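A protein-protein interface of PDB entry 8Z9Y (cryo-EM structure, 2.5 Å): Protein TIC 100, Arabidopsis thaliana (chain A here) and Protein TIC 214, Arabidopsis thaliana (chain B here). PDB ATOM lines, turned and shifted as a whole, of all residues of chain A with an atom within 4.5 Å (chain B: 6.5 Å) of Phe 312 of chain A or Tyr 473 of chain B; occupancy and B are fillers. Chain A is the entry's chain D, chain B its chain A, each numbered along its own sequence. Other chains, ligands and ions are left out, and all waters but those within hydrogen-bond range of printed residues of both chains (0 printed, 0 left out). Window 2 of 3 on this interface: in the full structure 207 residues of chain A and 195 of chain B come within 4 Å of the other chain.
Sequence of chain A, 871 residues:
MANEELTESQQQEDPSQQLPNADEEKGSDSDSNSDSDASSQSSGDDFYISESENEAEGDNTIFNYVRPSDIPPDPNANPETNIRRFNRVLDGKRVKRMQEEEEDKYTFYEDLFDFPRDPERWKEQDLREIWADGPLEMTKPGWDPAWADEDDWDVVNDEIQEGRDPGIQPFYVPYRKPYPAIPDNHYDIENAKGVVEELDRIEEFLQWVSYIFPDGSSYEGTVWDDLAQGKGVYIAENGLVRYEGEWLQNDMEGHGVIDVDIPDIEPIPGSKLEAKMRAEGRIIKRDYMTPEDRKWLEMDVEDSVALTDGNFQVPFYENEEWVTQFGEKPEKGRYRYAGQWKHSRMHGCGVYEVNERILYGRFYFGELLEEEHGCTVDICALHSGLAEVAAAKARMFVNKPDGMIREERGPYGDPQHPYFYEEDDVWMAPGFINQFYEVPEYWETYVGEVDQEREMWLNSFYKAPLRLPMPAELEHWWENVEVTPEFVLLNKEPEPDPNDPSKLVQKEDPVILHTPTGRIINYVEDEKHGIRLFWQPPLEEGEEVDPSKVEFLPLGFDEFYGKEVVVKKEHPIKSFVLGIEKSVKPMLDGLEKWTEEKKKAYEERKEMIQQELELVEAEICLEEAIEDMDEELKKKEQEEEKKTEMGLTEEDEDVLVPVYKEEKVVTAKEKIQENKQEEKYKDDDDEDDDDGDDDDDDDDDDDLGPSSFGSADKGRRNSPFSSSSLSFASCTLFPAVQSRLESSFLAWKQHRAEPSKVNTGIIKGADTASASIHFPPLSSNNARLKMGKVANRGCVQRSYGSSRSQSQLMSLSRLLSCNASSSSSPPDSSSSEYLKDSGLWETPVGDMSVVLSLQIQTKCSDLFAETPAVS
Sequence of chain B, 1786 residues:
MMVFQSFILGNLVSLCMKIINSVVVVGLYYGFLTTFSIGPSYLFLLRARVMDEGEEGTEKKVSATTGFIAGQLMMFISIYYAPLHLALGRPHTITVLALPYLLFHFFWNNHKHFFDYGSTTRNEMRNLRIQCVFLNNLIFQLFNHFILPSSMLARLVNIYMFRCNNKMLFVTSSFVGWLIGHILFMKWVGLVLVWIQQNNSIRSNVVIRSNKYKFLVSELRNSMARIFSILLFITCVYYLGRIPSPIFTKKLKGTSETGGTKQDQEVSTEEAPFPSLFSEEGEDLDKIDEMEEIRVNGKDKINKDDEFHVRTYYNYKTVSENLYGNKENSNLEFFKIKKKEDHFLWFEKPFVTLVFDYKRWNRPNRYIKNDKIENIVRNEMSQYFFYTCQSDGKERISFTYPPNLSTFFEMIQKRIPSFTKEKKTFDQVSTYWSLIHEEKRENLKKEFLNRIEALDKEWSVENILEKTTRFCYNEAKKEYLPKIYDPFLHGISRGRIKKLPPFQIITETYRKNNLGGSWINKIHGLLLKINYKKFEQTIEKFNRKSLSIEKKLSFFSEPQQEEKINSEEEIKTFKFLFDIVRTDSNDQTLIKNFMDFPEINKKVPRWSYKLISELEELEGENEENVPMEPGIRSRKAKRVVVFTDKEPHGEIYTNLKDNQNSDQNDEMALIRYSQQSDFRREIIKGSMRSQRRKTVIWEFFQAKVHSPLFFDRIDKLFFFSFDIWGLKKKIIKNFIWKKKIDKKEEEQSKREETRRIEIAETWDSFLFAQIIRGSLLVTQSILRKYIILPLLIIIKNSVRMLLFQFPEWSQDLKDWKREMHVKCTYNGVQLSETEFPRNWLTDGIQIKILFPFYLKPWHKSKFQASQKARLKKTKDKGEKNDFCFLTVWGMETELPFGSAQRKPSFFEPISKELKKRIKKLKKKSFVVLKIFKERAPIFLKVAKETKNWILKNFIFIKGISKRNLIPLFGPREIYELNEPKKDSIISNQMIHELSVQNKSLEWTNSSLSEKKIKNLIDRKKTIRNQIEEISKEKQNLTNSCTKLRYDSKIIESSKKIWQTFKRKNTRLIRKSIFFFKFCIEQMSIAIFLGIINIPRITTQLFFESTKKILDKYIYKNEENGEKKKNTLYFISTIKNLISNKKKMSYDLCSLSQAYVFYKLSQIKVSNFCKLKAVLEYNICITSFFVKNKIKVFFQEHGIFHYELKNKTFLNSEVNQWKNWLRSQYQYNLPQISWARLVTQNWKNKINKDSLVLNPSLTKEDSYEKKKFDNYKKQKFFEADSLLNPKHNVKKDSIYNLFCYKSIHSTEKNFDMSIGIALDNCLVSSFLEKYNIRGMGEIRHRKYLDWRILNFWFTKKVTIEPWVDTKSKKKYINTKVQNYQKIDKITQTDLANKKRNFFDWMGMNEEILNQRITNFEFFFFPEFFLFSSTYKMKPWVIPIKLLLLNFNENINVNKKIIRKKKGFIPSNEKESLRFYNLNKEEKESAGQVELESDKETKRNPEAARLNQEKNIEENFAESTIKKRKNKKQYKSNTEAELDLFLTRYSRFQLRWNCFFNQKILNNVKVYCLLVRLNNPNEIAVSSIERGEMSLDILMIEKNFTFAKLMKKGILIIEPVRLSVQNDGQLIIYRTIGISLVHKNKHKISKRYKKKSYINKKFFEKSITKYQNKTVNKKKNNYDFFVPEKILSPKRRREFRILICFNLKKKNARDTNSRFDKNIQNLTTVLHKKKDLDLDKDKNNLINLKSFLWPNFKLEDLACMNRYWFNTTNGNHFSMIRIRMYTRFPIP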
ATOM      1  N   ILE A 268      -0.583  31.015 -19.906  1.00  0.00           N
ATOM      2  CA  ILE A 268       0.271  31.366 -18.767  1.00  0.00           C
ATOM      3  C   ILE A 268       1.731  31.269 -19.196  1.00  0.00           C
ATOM      4  O   ILE A 268       2.108  30.298 -19.876  1.00  0.00           O
ATOM      5  CB  ILE A 268      -0.023  30.445 -17.579  1.00  0.00           C
ATOM      6  CG1 ILE A 268      -1.160  31.020 -16.734  1.00  0.00           C
ATOM      7  CG2 ILE A 268       1.218  30.239 -16.724  1.00  0.00           C
ATOM      8  CD1 ILE A 268      -1.572  30.134 -15.583  1.00  0.00           C
ATOM      9  N   THR A 308      -3.936  32.265  -5.753  1.00  0.00           N
ATOM     10  CA  THR A 308      -5.167  31.541  -6.054  1.00  0.00           C
ATOM     11  C   THR A 308      -5.203  30.172  -5.384  1.00  0.00           C
ATOM     12  O   THR A 308      -6.268  29.730  -4.937  1.00  0.00           O
ATOM     13  CB  THR A 308      -5.324  31.397  -7.569  1.00  0.00           C
ATOM     14  OG1 THR A 308      -5.533  32.689  -8.152  1.00  0.00           O
ATOM     15  CG2 THR A 308      -6.499  30.500  -7.913  1.00  0.00           C
ATOM     16  N   ASP A 309      -4.055  29.498  -5.293  1.00  0.00           N
ATOM     17  CA  ASP A 309      -3.940  28.140  -4.751  1.00  0.00           C
ATOM     18  C   ASP A 309      -4.711  27.206  -5.677  1.00  0.00           C
ATOM     19  O   ASP A 309      -4.403  27.173  -6.880  1.00  0.00           O
ATOM     20  CB  ASP A 309      -4.372  28.126  -3.282  1.00  0.00           C
ATOM     21  CG  ASP A 309      -3.245  28.494  -2.340  1.00  0.00           C
ATOM     22  OD1 ASP A 309      -2.070  28.285  -2.709  1.00  0.00           O
ATOM     23  OD2 ASP A 309      -3.534  28.988  -1.230  1.00  0.00           O
ATOM     24  N   GLY A 310      -5.689  26.445  -5.193  1.00  0.00           N
ATOM     25  CA  GLY A 310      -6.394  25.503  -6.038  1.00  0.00           C
ATOM     26  C   GLY A 310      -7.799  25.931  -6.410  1.00  0.00           C
ATOM     27  O   GLY A 310      -8.602  25.110  -6.863  1.00  0.00           O
ATOM     28  N   ASN A 311      -8.110  27.212  -6.226  1.00  0.00           N
ATOM     29  CA  ASN A 311      -9.451  27.727  -6.504  1.00  0.00           C
ATOM     30  C   ASN A 311      -9.519  28.244  -7.941  1.00  0.00           C
ATOM     31  O   ASN A 311      -9.543  29.446  -8.214  1.00  0.00           O
ATOM     32  CB  ASN A 311      -9.823  28.809  -5.499  1.00  0.00           C
ATOM     33  CG  ASN A 311      -9.888  28.285  -4.081  1.00  0.00           C
ATOM     34  OD1 ASN A 311      -9.528  27.140  -3.814  1.00  0.00           O
ATOM     35  ND2 ASN A 311     -10.349  29.124  -3.161  1.00  0.00           N
ATOM     36  N   PHE A 312      -9.562  27.297  -8.872  1.00  0.00           N
ATOM     37  CA  PHE A 312      -9.680  27.598 -10.291  1.00  0.00           C
ATOM     38  C   PHE A 312     -11.140  27.496 -10.706  1.00  0.00           C
ATOM     39  O   PHE A 312     -11.810  26.503 -10.401  1.00  0.00           O
ATOM     40  CB  PHE A 312      -8.813  26.653 -11.123  1.00  0.00           C
ATOM     41  CG  PHE A 312      -7.352  26.736 -10.798  1.00  0.00           C
ATOM     42  CD1 PHE A 312      -6.668  27.930 -10.936  1.00  0.00           C
ATOM     43  CD2 PHE A 312      -6.663  25.623 -10.349  1.00  0.00           C
ATOM     44  CE1 PHE A 312      -5.323  28.012 -10.635  1.00  0.00           C
ATOM     45  CE2 PHE A 312      -5.320  25.700 -10.047  1.00  0.00           C
ATOM     46  CZ  PHE A 312      -4.649  26.895 -10.190  1.00  0.00           C
ATOM     47  N   GLN A 313     -11.626  28.518 -11.399  1.00  0.00           N
ATOM     48  CA  GLN A 313     -13.042  28.660 -11.700  1.00  0.00           C
ATOM     49  C   GLN A 313     -13.342  28.285 -13.145  1.00  0.00           C
ATOM     50  O   GLN A 313     -12.474  28.323 -14.021  1.00  0.00           O
ATOM     51  CB  GLN A 313     -13.502  30.095 -11.434  1.00  0.00           C
ATOM     52  CG  GLN A 313     -13.153  30.611 -10.052  1.00  0.00           C
ATOM     53  CD  GLN A 313     -14.061  30.053  -8.979  1.00  0.00           C
ATOM     54  OE1 GLN A 313     -15.201  30.490  -8.827  1.00  0.00           O
ATOM     55  NE2 GLN A 313     -13.560  29.080  -8.229  1.00  0.00           N
ATOM     56  N   VAL A 314     -14.593  27.916 -13.381  1.00  0.00           N
ATOM     57  CA  VAL A 314     -15.132  27.664 -14.713  1.00  0.00           C
ATOM     58  C   VAL A 314     -16.126  28.777 -15.025  1.00  0.00           C
ATOM     59  O   VAL A 314     -17.149  28.892 -14.337  1.00  0.00           O
ATOM     60  CB  VAL A 314     -15.801  26.285 -14.808  1.00  0.00           C
ATOM     61  CG1 VAL A 314     -16.473  26.115 -16.158  1.00  0.00           C
ATOM     62  CG2 VAL A 314     -14.781  25.185 -14.575  1.00  0.00           C
ATOM     63  N   PHE B 471      -6.286  34.786 -18.613  1.00  0.00           N
ATOM     64  CA  PHE B 471      -5.297  33.745 -18.371  1.00  0.00           C
ATOM     65  C   PHE B 471      -5.985  32.423 -18.063  1.00  0.00           C
ATOM     66  O   PHE B 471      -6.850  32.348 -17.185  1.00  0.00           O
ATOM     67  CB  PHE B 471      -4.376  34.148 -17.223  1.00  0.00           C
ATOM     68  CG  PHE B 471      -3.354  35.177 -17.604  1.00  0.00           C
ATOM     69  CD1 PHE B 471      -2.127  34.795 -18.115  1.00  0.00           C
ATOM     70  CD2 PHE B 471      -3.623  36.526 -17.459  1.00  0.00           C
ATOM     71  CE1 PHE B 471      -1.187  35.740 -18.470  1.00  0.00           C
ATOM     72  CE2 PHE B 471      -2.687  37.474 -17.812  1.00  0.00           C
ATOM     73  CZ  PHE B 471      -1.468  37.080 -18.319  1.00  0.00           C
ATOM     74  N   CYS B 472      -5.599  31.379 -18.789  1.00  0.00           N
ATOM     75  CA  CYS B 472      -6.155  30.046 -18.619  1.00  0.00           C
ATOM     76  C   CYS B 472      -5.108  29.129 -18.005  1.00  0.00           C
ATOM     77  O   CYS B 472      -3.949  29.124 -18.429  1.00  0.00           O
ATOM     78  CB  CYS B 472      -6.632  29.472 -19.955  1.00  0.00           C
ATOM     79  SG  CYS B 472      -6.969  27.697 -19.920  1.00  0.00           S
ATOM     80  N   TYR B 473      -5.524  28.354 -17.006  1.00  0.00           N
ATOM     81  CA  TYR B 473      -4.623  27.463 -16.288  1.00  0.00           C
ATOM     82  C   TYR B 473      -4.619  26.044 -16.838  1.00  0.00           C
ATOM     83  O   TYR B 473      -3.571  25.392 -16.849  1.00  0.00           O
ATOM     84  CB  TYR B 473      -4.991  27.427 -14.802  1.00  0.00           C
ATOM     85  CG  TYR B 473      -4.048  26.601 -13.959  1.00  0.00           C
ATOM     86  CD1 TYR B 473      -2.815  27.102 -13.569  1.00  0.00           C
ATOM     87  CD2 TYR B 473      -4.391  25.319 -13.554  1.00  0.00           C
ATOM     88  CE1 TYR B 473      -1.950  26.353 -12.799  1.00  0.00           C
ATOM     89  CE2 TYR B 473      -3.533  24.561 -12.784  1.00  0.00           C
ATOM     90  CZ  TYR B 473      -2.314  25.082 -12.409  1.00  0.00           C
ATOM     91  OH  TYR B 473      -1.457  24.329 -11.642  1.00  0.00           O
ATOM     92  N   ASN B 474      -5.767  25.548 -17.294  1.00  0.00           N
ATOM     93  CA  ASN B 474      -5.862  24.183 -17.807  1.00  0.00           C
ATOM     94  C   ASN B 474      -7.039  24.122 -18.768  1.00  0.00           C
ATOM     95  O   ASN B 474      -8.193  24.179 -18.337  1.00  0.00           O
ATOM     96  CB  ASN B 474      -6.029  23.182 -16.667  1.00  0.00           C
ATOM     97  CG  ASN B 474      -6.027  21.746 -17.149  1.00  0.00           C
ATOM     98  OD1 ASN B 474      -5.685  21.463 -18.297  1.00  0.00           O
ATOM     99  ND2 ASN B 474      -6.411  20.828 -16.270  1.00  0.00           N
ATOM    100  N   GLU B 475      -6.746  24.003 -20.064  1.00  0.00           N
ATOM    101  CA  GLU B 475      -7.808  23.934 -21.061  1.00  0.00           C
ATOM    102  C   GLU B 475      -8.503  22.580 -21.078  1.00  0.00           C
ATOM    103  O   GLU B 475      -9.601  22.471 -21.634  1.00  0.00           O
ATOM    104  CB  GLU B 475      -7.250  24.249 -22.449  1.00  0.00           C
ATOM    105  CG  GLU B 475      -7.398  25.706 -22.857  1.00  0.00           C
ATOM    106  CD  GLU B 475      -7.344  25.901 -24.358  1.00  0.00           C
ATOM    107  OE1 GLU B 475      -6.914  24.967 -25.065  1.00  0.00           O
ATOM    108  OE2 GLU B 475      -7.733  26.989 -24.830  1.00  0.00           O
ATOM    109  N   GLU B 479     -10.430  25.348 -16.621  1.00  0.00           N
ATOM    110  CA  GLU B 479     -10.289  25.984 -15.319  1.00  0.00           C
ATOM    111  C   GLU B 479      -9.389  27.206 -15.454  1.00  0.00           C
ATOM    112  O   GLU B 479      -8.210  27.078 -15.798  1.00  0.00           O
ATOM    113  CB  GLU B 479      -9.719  25.004 -14.295  1.00  0.00           C
ATOM    114  CG  GLU B 479     -10.764  24.096 -13.672  1.00  0.00           C
ATOM    115  CD  GLU B 479     -10.278  23.437 -12.398  1.00  0.00           C
ATOM    116  OE1 GLU B 479      -9.048  23.391 -12.184  1.00  0.00           O
ATOM    117  OE2 GLU B 479     -11.124  22.966 -11.611  1.00  0.00           O
ATOM    118  N   TYR B 480      -9.946  28.380 -15.179  1.00  0.00           N
ATOM    119  CA  TYR B 480      -9.241  29.646 -15.298  1.00  0.00           C
ATOM    120  C   TYR B 480      -8.952  30.202 -13.907  1.00  0.00           C
ATOM    121  O   TYR B 480      -9.383  29.657 -12.889  1.00  0.00           O
ATOM    122  CB  TYR B 480     -10.053  30.659 -16.114  1.00  0.00           C
ATOM    123  CG  TYR B 480     -10.505  30.218 -17.494  1.00  0.00           C
ATOM    124  CD1 TYR B 480     -10.074  29.022 -18.057  1.00  0.00           C
ATOM    125  CD2 TYR B 480     -11.371  31.007 -18.235  1.00  0.00           C
ATOM    126  CE1 TYR B 480     -10.494  28.630 -19.310  1.00  0.00           C
ATOM    127  CE2 TYR B 480     -11.794  30.624 -19.489  1.00  0.00           C
ATOM    128  CZ  TYR B 480     -11.354  29.436 -20.022  1.00  0.00           C
ATOM    129  OH  TYR B 480     -11.778  29.054 -21.271  1.00  0.00           O
ATOM    130  N   LEU B 481      -8.210  31.304 -13.874  1.00  0.00           N
ATOM    131  CA  LEU B 481      -8.021  32.029 -12.632  1.00  0.00           C
ATOM    132  C   LEU B 481      -9.299  32.786 -12.275  1.00  0.00           C
ATOM    133  O   LEU B 481     -10.075  33.156 -13.160  1.00  0.00           O
ATOM    134  CB  LEU B 481      -6.860  33.009 -12.750  1.00  0.00           C
ATOM    135  CG  LEU B 481      -5.468  32.436 -13.011  1.00  0.00           C
ATOM    136  CD1 LEU B 481      -4.415  33.510 -12.814  1.00  0.00           C
ATOM    137  CD2 LEU B 481      -5.202  31.252 -12.103  1.00  0.00           C
ATOM    138  N   PRO B 482      -9.550  33.015 -10.988  1.00  0.00           N
ATOM    139  CA  PRO B 482     -10.682  33.866 -10.607  1.00  0.00           C
ATOM    140  C   PRO B 482     -10.534  35.251 -11.217  1.00  0.00           C
ATOM    141  O   PRO B 482      -9.436  35.803 -11.290  1.00  0.00           O
ATOM    142  CB  PRO B 482     -10.597  33.907  -9.078  1.00  0.00           C
ATOM    143  CG  PRO B 482      -9.876  32.662  -8.711  1.00  0.00           C
ATOM    144  CD  PRO B 482      -8.894  32.410  -9.816  1.00  0.00           C
ATOM    145  N   ILE B1450     -16.883  31.197  -6.336  1.00  0.00           N
ATOM    146  CA  ILE B1450     -17.482  30.033  -5.692  1.00  0.00           C
ATOM    147  C   ILE B1450     -16.596  29.528  -4.561  1.00  0.00           C
ATOM    148  O   ILE B1450     -17.094  28.959  -3.581  1.00  0.00           O
ATOM    149  CB  ILE B1450     -17.775  28.932  -6.735  1.00  0.00           C
ATOM    150  CG1 ILE B1450     -18.909  28.027  -6.255  1.00  0.00           C
ATOM    151  CG2 ILE B1450     -16.533  28.108  -7.037  1.00  0.00           C
ATOM    152  CD1 ILE B1450     -19.542  27.210  -7.361  1.00  0.00           C
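Tyr 473 of chain B touches just these residues of chain A: Ile 268 (3.8 Å) and Phe 312 (3.5 Å).
Of the printed residues of chain A, Glu 479 of chain B touches Phe 312 and Gln 313.
Printed residues of chain A within 4 Å of Cys 472 of chain B: Ile 268 (3.8 Å).
Of the printed residues of chain B, Gln 313 of chain A touches Glu 479, Tyr 480 and Ile 1450.
Of the printed residues of chain A, Leu 481 of chain B touches Phe 312 (3.6 Å).
The nearest printed residue of chain A that does not touch Tyr 473 of chain B is Asp 309 of chain A (6.3 Å).
The nearest printed residue of chain A that does not touch Tyr 480 of chain B is Asn 311 of chain A (4.7 Å).
Among the printed residues, merely in contact across the chains: Ile 268 of chain A with Cys 472 of chain B, Ile 268 of chain A with Tyr 473 of chain B, Thr 308 of chain A with Pro 482 of chain B, Asn 311 of chain A with Pro 482 of chain B, Phe 312 of chain A with Tyr 473 of chain B, Phe 312 of chain A with Glu 479 of chain B, Phe 312 of chain A with Tyr 480 of chain B, Phe 312 of chain A with Leu 481 of chain B and Gln 313 of chain A with Glu 479 of chain B.
The backbone NH (N) of Tyr 480 of chain B sits at hydrogen-bond distance from the backbone carbonyl oxygen (O) of Gln 313 of chain A, at 2.8 Å.
OE1 of Gln 313 of chain A is in hydrogen-bond range of N of Ile 1450 of chain B (3.1 Å).
The backbone carbonyl oxygen (O) of Glu 479 of chain B sits at hydrogen-bond distance from the backbone NH (N) of Tyr 473 of chain B, 3.2 Å away.
SG of Cys 472 of chain B is in hydrogen-bond range of N of Asn 474 of chain B.
The side-chain sulfur (SG) of Cys 472 of chain B lies close to the backbone NH (N) of Glu 475 of chain B (3.7 Å).
The backbone NH (N) of Glu 479 of chain B lies within hydrogen-bond range of the backbone carbonyl oxygen (O) of Asn 474 of chain B (3.1 Å).
Printed residues of chain A that touch a printed residue of chain B: Ile 268, Thr 308, Asn 311, Phe 312 and Gln 313.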
